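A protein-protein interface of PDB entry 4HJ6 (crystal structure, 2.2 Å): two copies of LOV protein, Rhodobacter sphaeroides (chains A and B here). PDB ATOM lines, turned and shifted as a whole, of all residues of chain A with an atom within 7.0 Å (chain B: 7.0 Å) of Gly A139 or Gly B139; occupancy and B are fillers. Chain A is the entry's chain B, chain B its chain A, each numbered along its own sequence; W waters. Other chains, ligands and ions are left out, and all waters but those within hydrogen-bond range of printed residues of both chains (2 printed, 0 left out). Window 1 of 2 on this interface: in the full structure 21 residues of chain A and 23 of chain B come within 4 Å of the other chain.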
ATOM      1  N   VAL A  20       5.423   6.489  13.531  1.00  0.00           N
ATOM      2  CA  VAL A  20       6.121   7.777  13.502  1.00  0.00           C
ATOM      3  C   VAL A  20       6.359   8.346  14.894  1.00  0.00           C
ATOM      4  O   VAL A  20       5.582   8.078  15.824  1.00  0.00           O
ATOM      5  CB  VAL A  20       5.355   8.829  12.694  1.00  0.00           C
ATOM      6  CG1 VAL A  20       5.223   8.390  11.249  1.00  0.00           C
ATOM      7  CG2 VAL A  20       3.982   9.091  13.322  1.00  0.00           C
ATOM      8  N   PHE A 102       6.250  18.698  12.971  1.00  0.00           N
ATOM      9  CA  PHE A 102       4.848  18.872  12.634  1.00  0.00           C
ATOM     10  C   PHE A 102       4.110  19.125  13.933  1.00  0.00           C
ATOM     11  O   PHE A 102       4.262  18.355  14.879  1.00  0.00           O
ATOM     12  CB  PHE A 102       4.298  17.566  12.055  1.00  0.00           C
ATOM     13  CG  PHE A 102       4.829  17.212  10.693  1.00  0.00           C
ATOM     14  CD1 PHE A 102       6.049  16.569  10.550  1.00  0.00           C
ATOM     15  CD2 PHE A 102       4.075  17.470   9.551  1.00  0.00           C
ATOM     16  CE1 PHE A 102       6.531  16.221   9.301  1.00  0.00           C
ATOM     17  CE2 PHE A 102       4.548  17.124   8.298  1.00  0.00           C
ATOM     18  CZ  PHE A 102       5.775  16.503   8.167  1.00  0.00           C
ATOM     19  N   ALA A 133      10.334  10.717   1.414  1.00  0.00           N
ATOM     20  CA  ALA A 133      10.336  10.225   2.787  1.00  0.00           C
ATOM     21  C   ALA A 133       9.513  11.132   3.699  1.00  0.00           C
ATOM     22  O   ALA A 133       8.670  10.655   4.477  1.00  0.00           O
ATOM     23  CB  ALA A 133      11.759  10.087   3.309  1.00  0.00           C
ATOM     24  N   ALA A 134       9.753  12.437   3.602  1.00  0.00           N
ATOM     25  CA  ALA A 134       9.025  13.399   4.414  1.00  0.00           C
ATOM     26  C   ALA A 134       7.525  13.357   4.093  1.00  0.00           C
ATOM     27  O   ALA A 134       6.687  13.362   5.005  1.00  0.00           O
ATOM     28  CB  ALA A 134       9.573  14.790   4.201  1.00  0.00           C
ATOM     29  N   ALA A 135       7.185  13.308   2.807  1.00  0.00           N
ATOM     30  CA  ALA A 135       5.780  13.223   2.412  1.00  0.00           C
ATOM     31  C   ALA A 135       5.158  11.927   2.937  1.00  0.00           C
ATOM     32  O   ALA A 135       3.981  11.901   3.300  1.00  0.00           O
ATOM     33  CB  ALA A 135       5.616  13.315   0.887  1.00  0.00           C
ATOM     34  N   GLY A 136       5.943  10.856   2.973  1.00  0.00           N
ATOM     35  CA  GLY A 136       5.460   9.585   3.487  1.00  0.00           C
ATOM     36  C   GLY A 136       5.178   9.710   4.973  1.00  0.00           C
ATOM     37  O   GLY A 136       4.122   9.259   5.452  1.00  0.00           O
ATOM     38  N   HIS A 137       6.123  10.312   5.704  1.00  0.00           N
ATOM     39  CA  HIS A 137       5.925  10.576   7.119  1.00  0.00           C
ATOM     40  C   HIS A 137       4.625  11.352   7.313  1.00  0.00           C
ATOM     41  O   HIS A 137       3.815  11.024   8.188  1.00  0.00           O
ATOM     42  CB  HIS A 137       7.098  11.377   7.682  1.00  0.00           C
ATOM     43  CG  HIS A 137       6.936  11.747   9.113  1.00  0.00           C
ATOM     44  ND1 HIS A 137       7.698  11.180  10.124  1.00  0.00           N
ATOM     45  CD2 HIS A 137       6.109  12.622   9.729  1.00  0.00           C
ATOM     46  CE1 HIS A 137       7.343  11.692  11.281  1.00  0.00           C
ATOM     47  NE2 HIS A 137       6.384  12.581  11.071  1.00  0.00           N
ATOM     48  N   ALA A 138       4.410  12.370   6.488  1.00  0.00           N
ATOM     49  CA  ALA A 138       3.226  13.208   6.659  1.00  0.00           C
ATOM     50  C   ALA A 138       1.924  12.422   6.429  1.00  0.00           C
ATOM     51  O   ALA A 138       0.898  12.688   7.080  1.00  0.00           O
ATOM     52  CB  ALA A 138       3.299  14.407   5.736  1.00  0.00           C
ATOM     53  N   GLY A 139       1.959  11.464   5.505  1.00  0.00           N
ATOM     54  CA  GLY A 139       0.782  10.654   5.221  1.00  0.00           C
ATOM     55  C   GLY A 139       0.471   9.716   6.372  1.00  0.00           C
ATOM     56  O   GLY A 139      -0.693   9.533   6.740  1.00  0.00           O
ATOM     57  N   ALA A 140       1.517   9.111   6.931  1.00  0.00           N
ATOM     58  CA  ALA A 140       1.385   8.264   8.107  1.00  0.00           C
ATOM     59  C   ALA A 140       0.869   9.092   9.283  1.00  0.00           C
ATOM     60  O   ALA A 140      -0.053   8.669   9.985  1.00  0.00           O
ATOM     61  CB  ALA A 140       2.728   7.620   8.464  1.00  0.00           C
ATOM     62  N   LEU A 141       1.478  10.255   9.513  1.00  0.00           N
ATOM     63  CA  LEU A 141       1.028  11.150  10.578  1.00  0.00           C
ATOM     64  C   LEU A 141      -0.456  11.467  10.452  1.00  0.00           C
ATOM     65  O   LEU A 141      -1.200  11.396  11.438  1.00  0.00           O
ATOM     66  CB  LEU A 141       1.821  12.461  10.560  1.00  0.00           C
ATOM     67  CG  LEU A 141       1.358  13.544  11.555  1.00  0.00           C
ATOM     68  CD1 LEU A 141       1.419  13.059  13.011  1.00  0.00           C
ATOM     69  CD2 LEU A 141       2.196  14.801  11.410  1.00  0.00           C
ATOM     70  N   THR A 142      -0.888  11.821   9.242  1.00  0.00           N
ATOM     71  CA  THR A 142      -2.277  12.228   9.031  1.00  0.00           C
ATOM     72  C   THR A 142      -3.202  11.066   9.360  1.00  0.00           C
ATOM     73  O   THR A 142      -4.313  11.265   9.879  1.00  0.00           O
ATOM     74  CB  THR A 142      -2.519  12.721   7.586  1.00  0.00           C
ATOM     75  OG1 THR A 142      -1.560  13.736   7.275  1.00  0.00           O
ATOM     76  CG2 THR A 142      -3.904  13.331   7.452  1.00  0.00           C
ATOM     77  N   GLY A 143      -2.740   9.849   9.086  1.00  0.00           N
ATOM     78  CA  GLY A 143      -3.488   8.671   9.484  1.00  0.00           C
ATOM     79  C   GLY A 143      -3.657   8.605  10.992  1.00  0.00           C
ATOM     80  O   GLY A 143      -4.735   8.271  11.487  1.00  0.00           O
ATOM     81  N   GLU A 144      -2.588   8.906  11.732  1.00  0.00           N
ATOM     82  CA  GLU A 144      -2.657   8.847  13.185  1.00  0.00           C
ATOM     83  C   GLU A 144      -3.529   9.974  13.742  1.00  0.00           C
ATOM     84  O   GLU A 144      -4.289   9.770  14.684  1.00  0.00           O
ATOM     85  CB  GLU A 144      -1.241   8.876  13.779  1.00  0.00           C
ATOM     86  CG  GLU A 144      -0.374   7.682  13.319  1.00  0.00           C
ATOM     87  CD  GLU A 144      -0.644   6.437  14.144  1.00  0.00           C
ATOM     88  OE1 GLU A 144      -0.296   6.454  15.344  1.00  0.00           O
ATOM     89  OE2 GLU A 144      -1.173   5.440  13.629  1.00  0.00           O
ATOM     90  N   GLU A 156      -9.404  13.755   5.970  1.00  0.00           N
ATOM     91  CA  GLU A 156      -8.109  13.089   6.042  1.00  0.00           C
ATOM     92  C   GLU A 156      -7.313  13.233   4.740  1.00  0.00           C
ATOM     93  O   GLU A 156      -6.154  13.658   4.767  1.00  0.00           O
ATOM     94  CB  GLU A 156      -8.234  11.611   6.442  1.00  0.00           C
ATOM     95  CG  GLU A 156      -6.856  10.990   6.711  1.00  0.00           C
ATOM     96  CD  GLU A 156      -6.897   9.524   7.117  1.00  0.00           C
ATOM     97  OE1 GLU A 156      -7.984   9.036   7.514  1.00  0.00           O
ATOM     98  OE2 GLU A 156      -5.825   8.865   7.044  1.00  0.00           O
ATOM     99  N   ARG A 160      -3.800  15.299   4.368  1.00  0.00           N
ATOM    100  CA  ARG A 160      -2.603  14.596   3.929  1.00  0.00           C
ATOM    101  C   ARG A 160      -1.986  15.249   2.697  1.00  0.00           C
ATOM    102  O   ARG A 160      -0.772  15.491   2.670  1.00  0.00           O
ATOM    103  CB  ARG A 160      -2.904  13.128   3.642  1.00  0.00           C
ATOM    104  CG  ARG A 160      -1.779  12.389   2.916  1.00  0.00           C
ATOM    105  CD  ARG A 160      -2.361  11.194   2.174  1.00  0.00           C
ATOM    106  NE  ARG A 160      -3.254  10.479   3.068  1.00  0.00           N
ATOM    107  CZ  ARG A 160      -4.491  10.105   2.782  1.00  0.00           C
ATOM    108  NH1 ARG A 160      -5.011  10.334   1.583  1.00  0.00           N
ATOM    109  NH2 ARG A 160      -5.203   9.477   3.703  1.00  0.00           N
ATOM    110  N   LEU A 163      -0.579  18.411   3.708  1.00  0.00           N
ATOM    111  CA  LEU A 163       0.509  18.178   4.660  1.00  0.00           C
ATOM    112  C   LEU A 163       1.738  17.607   3.951  1.00  0.00           C
ATOM    113  O   LEU A 163       2.862  18.071   4.167  1.00  0.00           O
ATOM    114  CB  LEU A 163       0.079  17.244   5.778  1.00  0.00           C
ATOM    115  CG  LEU A 163       0.945  17.443   7.002  1.00  0.00           C
ATOM    116  CD1 LEU A 163       0.665  18.823   7.597  1.00  0.00           C
ATOM    117  CD2 LEU A 163       0.719  16.330   8.024  1.00  0.00           C
ATOM    118  N   ALA A 164       1.511  16.619   3.083  1.00  0.00           N
ATOM    119  CA  ALA A 164       2.581  16.051   2.264  1.00  0.00           C
ATOM    120  C   ALA A 164       3.249  17.114   1.387  1.00  0.00           C
ATOM    121  O   ALA A 164       4.469  17.087   1.184  1.00  0.00           O
ATOM    122  CB  ALA A 164       2.043  14.907   1.406  1.00  0.00           C
ATOM    123  N   VAL B  20      -7.676   6.345   2.919  1.00  0.00           N
ATOM    124  CA  VAL B  20      -7.241   6.059   1.547  1.00  0.00           C
ATOM    125  C   VAL B  20      -8.218   5.068   0.932  1.00  0.00           C
ATOM    126  O   VAL B  20      -8.829   4.270   1.652  1.00  0.00           O
ATOM    127  CB  VAL B  20      -5.813   5.468   1.474  1.00  0.00           C
ATOM    128  CG1 VAL B  20      -4.758   6.522   1.827  1.00  0.00           C
ATOM    129  CG2 VAL B  20      -5.683   4.248   2.399  1.00  0.00           C
ATOM    130  N   PHE B 102      -1.743   0.310  -5.690  1.00  0.00           N
ATOM    131  CA  PHE B 102      -0.875  -0.449  -4.787  1.00  0.00           C
ATOM    132  C   PHE B 102      -1.554  -1.768  -4.492  1.00  0.00           C
ATOM    133  O   PHE B 102      -2.738  -1.792  -4.140  1.00  0.00           O
ATOM    134  CB  PHE B 102      -0.708   0.269  -3.443  1.00  0.00           C
ATOM    135  CG  PHE B 102      -0.040   1.607  -3.543  1.00  0.00           C
ATOM    136  CD1 PHE B 102      -0.723   2.711  -4.032  1.00  0.00           C
ATOM    137  CD2 PHE B 102       1.283   1.763  -3.145  1.00  0.00           C
ATOM    138  CE1 PHE B 102      -0.092   3.951  -4.125  1.00  0.00           C
ATOM    139  CE2 PHE B 102       1.906   2.996  -3.239  1.00  0.00           C
ATOM    140  CZ  PHE B 102       1.226   4.087  -3.721  1.00  0.00           C
ATOM    141  N   ALA B 134       1.665  11.285  -3.781  1.00  0.00           N
ATOM    142  CA  ALA B 134       1.702   9.834  -3.914  1.00  0.00           C
ATOM    143  C   ALA B 134       2.495   9.227  -2.764  1.00  0.00           C
ATOM    144  O   ALA B 134       2.122   8.186  -2.211  1.00  0.00           O
ATOM    145  CB  ALA B 134       2.288   9.438  -5.256  1.00  0.00           C
ATOM    146  N   ALA B 135       3.595   9.871  -2.391  1.00  0.00           N
ATOM    147  CA  ALA B 135       4.349   9.397  -1.234  1.00  0.00           C
ATOM    148  C   ALA B 135       3.468   9.513   0.008  1.00  0.00           C
ATOM    149  O   ALA B 135       3.446   8.603   0.843  1.00  0.00           O
ATOM    150  CB  ALA B 135       5.663  10.165  -1.069  1.00  0.00           C
ATOM    151  N   GLY B 136       2.730  10.616   0.106  1.00  0.00           N
ATOM    152  CA  GLY B 136       1.754  10.800   1.169  1.00  0.00           C
ATOM    153  C   GLY B 136       0.800   9.623   1.271  1.00  0.00           C
ATOM    154  O   GLY B 136       0.621   9.046   2.347  1.00  0.00           O
ATOM    155  N   HIS B 137       0.218   9.244   0.136  1.00  0.00           N
ATOM    156  CA  HIS B 137      -0.708   8.117   0.059  1.00  0.00           C
ATOM    157  C   HIS B 137      -0.025   6.835   0.518  1.00  0.00           C
ATOM    158  O   HIS B 137      -0.566   6.082   1.340  1.00  0.00           O
ATOM    159  CB  HIS B 137      -1.221   7.976  -1.383  1.00  0.00           C
ATOM    160  CG  HIS B 137      -2.247   6.908  -1.558  1.00  0.00           C
ATOM    161  ND1 HIS B 137      -3.576   7.181  -1.793  1.00  0.00           N
ATOM    162  CD2 HIS B 137      -2.141   5.554  -1.521  1.00  0.00           C
ATOM    163  CE1 HIS B 137      -4.243   6.052  -1.910  1.00  0.00           C
ATOM    164  NE2 HIS B 137      -3.404   5.047  -1.750  1.00  0.00           N
ATOM    165  N   ALA B 138       1.197   6.607   0.036  1.00  0.00           N
ATOM    166  CA  ALA B 138       1.965   5.425   0.442  1.00  0.00           C
ATOM    167  C   ALA B 138       2.182   5.365   1.950  1.00  0.00           C
ATOM    168  O   ALA B 138       2.093   4.292   2.568  1.00  0.00           O
ATOM    169  CB  ALA B 138       3.302   5.391  -0.282  1.00  0.00           C
ATOM    170  N   GLY B 139       2.482   6.512   2.552  1.00  0.00           N
ATOM    171  CA  GLY B 139       2.690   6.562   3.991  1.00  0.00           C
ATOM    172  C   GLY B 139       1.397   6.239   4.725  1.00  0.00           C
ATOM    173  O   GLY B 139       1.413   5.485   5.681  1.00  0.00           O
ATOM    174  N   ALA B 140       0.274   6.801   4.268  1.00  0.00           N
ATOM    175  CA  ALA B 140      -1.014   6.505   4.873  1.00  0.00           C
ATOM    176  C   ALA B 140      -1.319   5.023   4.701  1.00  0.00           C
ATOM    177  O   ALA B 140      -1.752   4.350   5.647  1.00  0.00           O
ATOM    178  CB  ALA B 140      -2.122   7.360   4.238  1.00  0.00           C
ATOM    179  N   LEU B 141      -1.083   4.505   3.495  1.00  0.00           N
ATOM    180  CA  LEU B 141      -1.381   3.102   3.214  1.00  0.00           C
ATOM    181  C   LEU B 141      -0.572   2.154   4.097  1.00  0.00           C
ATOM    182  O   LEU B 141      -1.099   1.147   4.584  1.00  0.00           O
ATOM    183  CB  LEU B 141      -1.151   2.786   1.732  1.00  0.00           C
ATOM    184  CG  LEU B 141      -1.263   1.293   1.387  1.00  0.00           C
ATOM    185  CD1 LEU B 141      -2.662   0.759   1.664  1.00  0.00           C
ATOM    186  CD2 LEU B 141      -0.871   1.069  -0.057  1.00  0.00           C
ATOM    187  N   THR B 142       0.698   2.476   4.322  1.00  0.00           N
ATOM    188  CA  THR B 142       1.537   1.627   5.158  1.00  0.00           C
ATOM    189  C   THR B 142       0.980   1.567   6.575  1.00  0.00           C
ATOM    190  O   THR B 142       1.095   0.539   7.261  1.00  0.00           O
ATOM    191  CB  THR B 142       2.990   2.135   5.232  1.00  0.00           C
ATOM    192  OG1 THR B 142       3.540   2.226   3.912  1.00  0.00           O
ATOM    193  CG2 THR B 142       3.837   1.178   6.043  1.00  0.00           C
ATOM    194  N   GLY B 143       0.385   2.671   7.020  1.00  0.00           N
ATOM    195  CA  GLY B 143      -0.175   2.722   8.361  1.00  0.00           C
ATOM    196  C   GLY B 143      -1.275   1.687   8.444  1.00  0.00           C
ATOM    197  O   GLY B 143      -1.313   0.905   9.395  1.00  0.00           O
ATOM    198  N   GLU B 144      -2.147   1.670   7.436  1.00  0.00           N
ATOM    199  CA  GLU B 144      -3.263   0.717   7.393  1.00  0.00           C
ATOM    200  C   GLU B 144      -2.793  -0.736   7.303  1.00  0.00           C
ATOM    201  O   GLU B 144      -3.357  -1.611   7.949  1.00  0.00           O
ATOM    202  CB  GLU B 144      -4.220   1.028   6.227  1.00  0.00           C
ATOM    203  CG  GLU B 144      -4.566   2.510   6.011  1.00  0.00           C
ATOM    204  CD  GLU B 144      -5.411   3.124   7.135  1.00  0.00           C
ATOM    205  OE1 GLU B 144      -5.451   2.575   8.263  1.00  0.00           O
ATOM    206  OE2 GLU B 144      -6.020   4.194   6.889  1.00  0.00           O
ATOM    207  N   GLU B 156       7.387  -1.171  10.087  1.00  0.00           N
ATOM    208  CA  GLU B 156       6.510  -0.138   9.524  1.00  0.00           C
ATOM    209  C   GLU B 156       7.262   1.060   8.933  1.00  0.00           C
ATOM    210  O   GLU B 156       6.999   1.449   7.795  1.00  0.00           O
ATOM    211  CB  GLU B 156       5.459   0.343  10.540  1.00  0.00           C
ATOM    212  CG  GLU B 156       4.532   1.417   9.951  1.00  0.00           C
ATOM    213  CD  GLU B 156       3.398   1.836  10.880  1.00  0.00           C
ATOM    214  OE1 GLU B 156       3.142   1.141  11.887  1.00  0.00           O
ATOM    215  OE2 GLU B 156       2.755   2.870  10.590  1.00  0.00           O
ATOM    216  N   ARG B 160       7.498   1.921   5.042  1.00  0.00           N
ATOM    217  CA  ARG B 160       6.912   3.209   4.648  1.00  0.00           C
ATOM    218  C   ARG B 160       7.838   3.991   3.723  1.00  0.00           C
ATOM    219  O   ARG B 160       7.429   4.419   2.639  1.00  0.00           O
ATOM    220  CB  ARG B 160       6.547   4.081   5.858  1.00  0.00           C
ATOM    221  CG  ARG B 160       6.147   5.509   5.440  1.00  0.00           C
ATOM    222  CD  ARG B 160       5.646   6.358   6.592  1.00  0.00           C
ATOM    223  NE  ARG B 160       6.670   6.627   7.600  1.00  0.00           N
ATOM    224  CZ  ARG B 160       6.704   6.050   8.799  1.00  0.00           C
ATOM    225  NH1 ARG B 160       7.671   6.357   9.659  1.00  0.00           N
ATOM    226  NH2 ARG B 160       5.769   5.168   9.146  1.00  0.00           N
ATOM    227  N   ARG B 161       9.081   4.179   4.159  1.00  0.00           N
ATOM    228  CA  ARG B 161      10.066   4.918   3.379  1.00  0.00           C
ATOM    229  C   ARG B 161      10.249   4.305   1.987  1.00  0.00           C
ATOM    230  O   ARG B 161      10.279   5.014   0.982  1.00  0.00           O
ATOM    231  CB  ARG B 161      11.406   4.959   4.128  1.00  0.00           C
ATOM    232  CG  ARG B 161      12.472   5.853   3.486  1.00  0.00           C
ATOM    233  CD  ARG B 161      13.746   5.835   4.321  1.00  0.00           C
ATOM    234  NE  ARG B 161      13.455   5.379   5.681  1.00  0.00           N
ATOM    235  CZ  ARG B 161      14.011   5.872   6.780  1.00  0.00           C
ATOM    236  NH1 ARG B 161      13.666   5.385   7.967  1.00  0.00           N
ATOM    237  NH2 ARG B 161      14.909   6.845   6.692  1.00  0.00           N
ATOM    238  N   LEU B 163       8.123   2.193   0.317  1.00  0.00           N
ATOM    239  CA  LEU B 163       6.875   2.335  -0.450  1.00  0.00           C
ATOM    240  C   LEU B 163       6.738   3.757  -0.986  1.00  0.00           C
ATOM    241  O   LEU B 163       6.383   3.956  -2.143  1.00  0.00           O
ATOM    242  CB  LEU B 163       5.660   1.988   0.408  1.00  0.00           C
ATOM    243  CG  LEU B 163       4.615   1.002  -0.142  1.00  0.00           C
ATOM    244  CD1 LEU B 163       3.217   1.401   0.308  1.00  0.00           C
ATOM    245  CD2 LEU B 163       4.677   0.844  -1.652  1.00  0.00           C
ATOM    246  N   ALA B 164       7.041   4.735  -0.140  1.00  0.00           N
ATOM    247  CA  ALA B 164       7.017   6.146  -0.522  1.00  0.00           C
ATOM    248  C   ALA B 164       7.931   6.449  -1.703  1.00  0.00           C
ATOM    249  O   ALA B 164       7.570   7.241  -2.584  1.00  0.00           O
ATOM    250  CB  ALA B 164       7.412   7.020   0.670  1.00  0.00           C
HETATM  251  O   HOH W   1       0.634   3.186  12.329  1.00  0.00           O
HETATM  252  O   HOH W   2      -4.870   9.471  -1.751  1.00  0.00           O
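OE2 of Glu A156 is in salt-bridge range of NH2 of Arg A160 (3.5 Å).
Among the printed residues, pairs that only touch across the chains: Val A20 with Arg B160, Ala A135 with Ala B135, Ala A135 with Gly B136, Gly A136 with Ala B135, Gly A136 with Gly B139, Gly A136 with Arg B160, Gly A139 with Gly B136, Gly A139 with Gly B139, Gly A139 with Ala B140, Ala A140 with Gly B139, Ala A140 with Ala B140, Ala A140 with Arg B160, Arg A160 with Val B20, Arg A160 with Gly B136, Arg A160 with His B137 and Arg A160 with Ala B140.
Of chain B, only Gly B136 (3.3 Å), Gly B139 (3.96 Å) and Ala B140 (3.6 Å) come within 4 Å of Gly A139.
Gly B139 touches just these residues of chain A: Gly A136, Gly A139 and Ala A140.
Printed residues of chain A within 4 Å of Gly B136: Ala A135 (3.3 Å), Gly A139 (3.3 Å) and Arg A160 (3.6 Å).
Of the printed residues of chain A, Val B20 touches Arg A160.
Printed residues of chain A within 4 Å of Ala B140: Gly A139 (3.6 Å), Ala A140 (3.7 Å) and Arg A160 (3.5 Å).
Printed residues of chain B within 4 Å of Arg A160: Val B20 (3.5 Å), Gly B136 (3.6 Å), His B137 (3.8 Å) and Ala B140 (3.5 Å).
Leu B141 touches none of the printed residues of chain A.
Leu A141 touches none of the printed residues of chain B.
The nearest residue of chain B that does not touch Gly A139 is His B137 (5.3 Å).
Hydrophobic or aromatic side chains of chain B within 4 Å of the printed part of chain A: Val B20, Ala B135 and Ala B140.
Of the 18 printed residues of chain A, 6 touch a printed residue of chain B.
Along chain A the printed residues that touch a printed residue of chain B span positions 20 to 160.
Among the printed residues, no Asp or Glu carboxylate lies within 4 Å of a Lys or Arg side-chain nitrogen of the other chain.
Val A20 touches Arg B160, and with the chains exchanged Arg A160 touches Val B20.
Ala B135 touches its own counterpart, Ala A135.
Gly A136 touches Gly B139, and with the chains exchanged Gly A139 touches Gly B136.
Ala A140 touches Arg B160, and with the chains exchanged Arg A160 touches Ala B140.
Of the 16 pairs that touch across the chains among the printed residues, 15 have their exchanged pair printed and touching as well.
Water W2 bridges a ring nitrogen (ND1) of His B137 and the guanidinium group of Arg A160.
Water W1 bridges the side-chain carboxylate (OE2) of Glu B156 (2.8 Å) and the side-chain carboxylate (OE2) of Glu A144 (3.2 Å).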
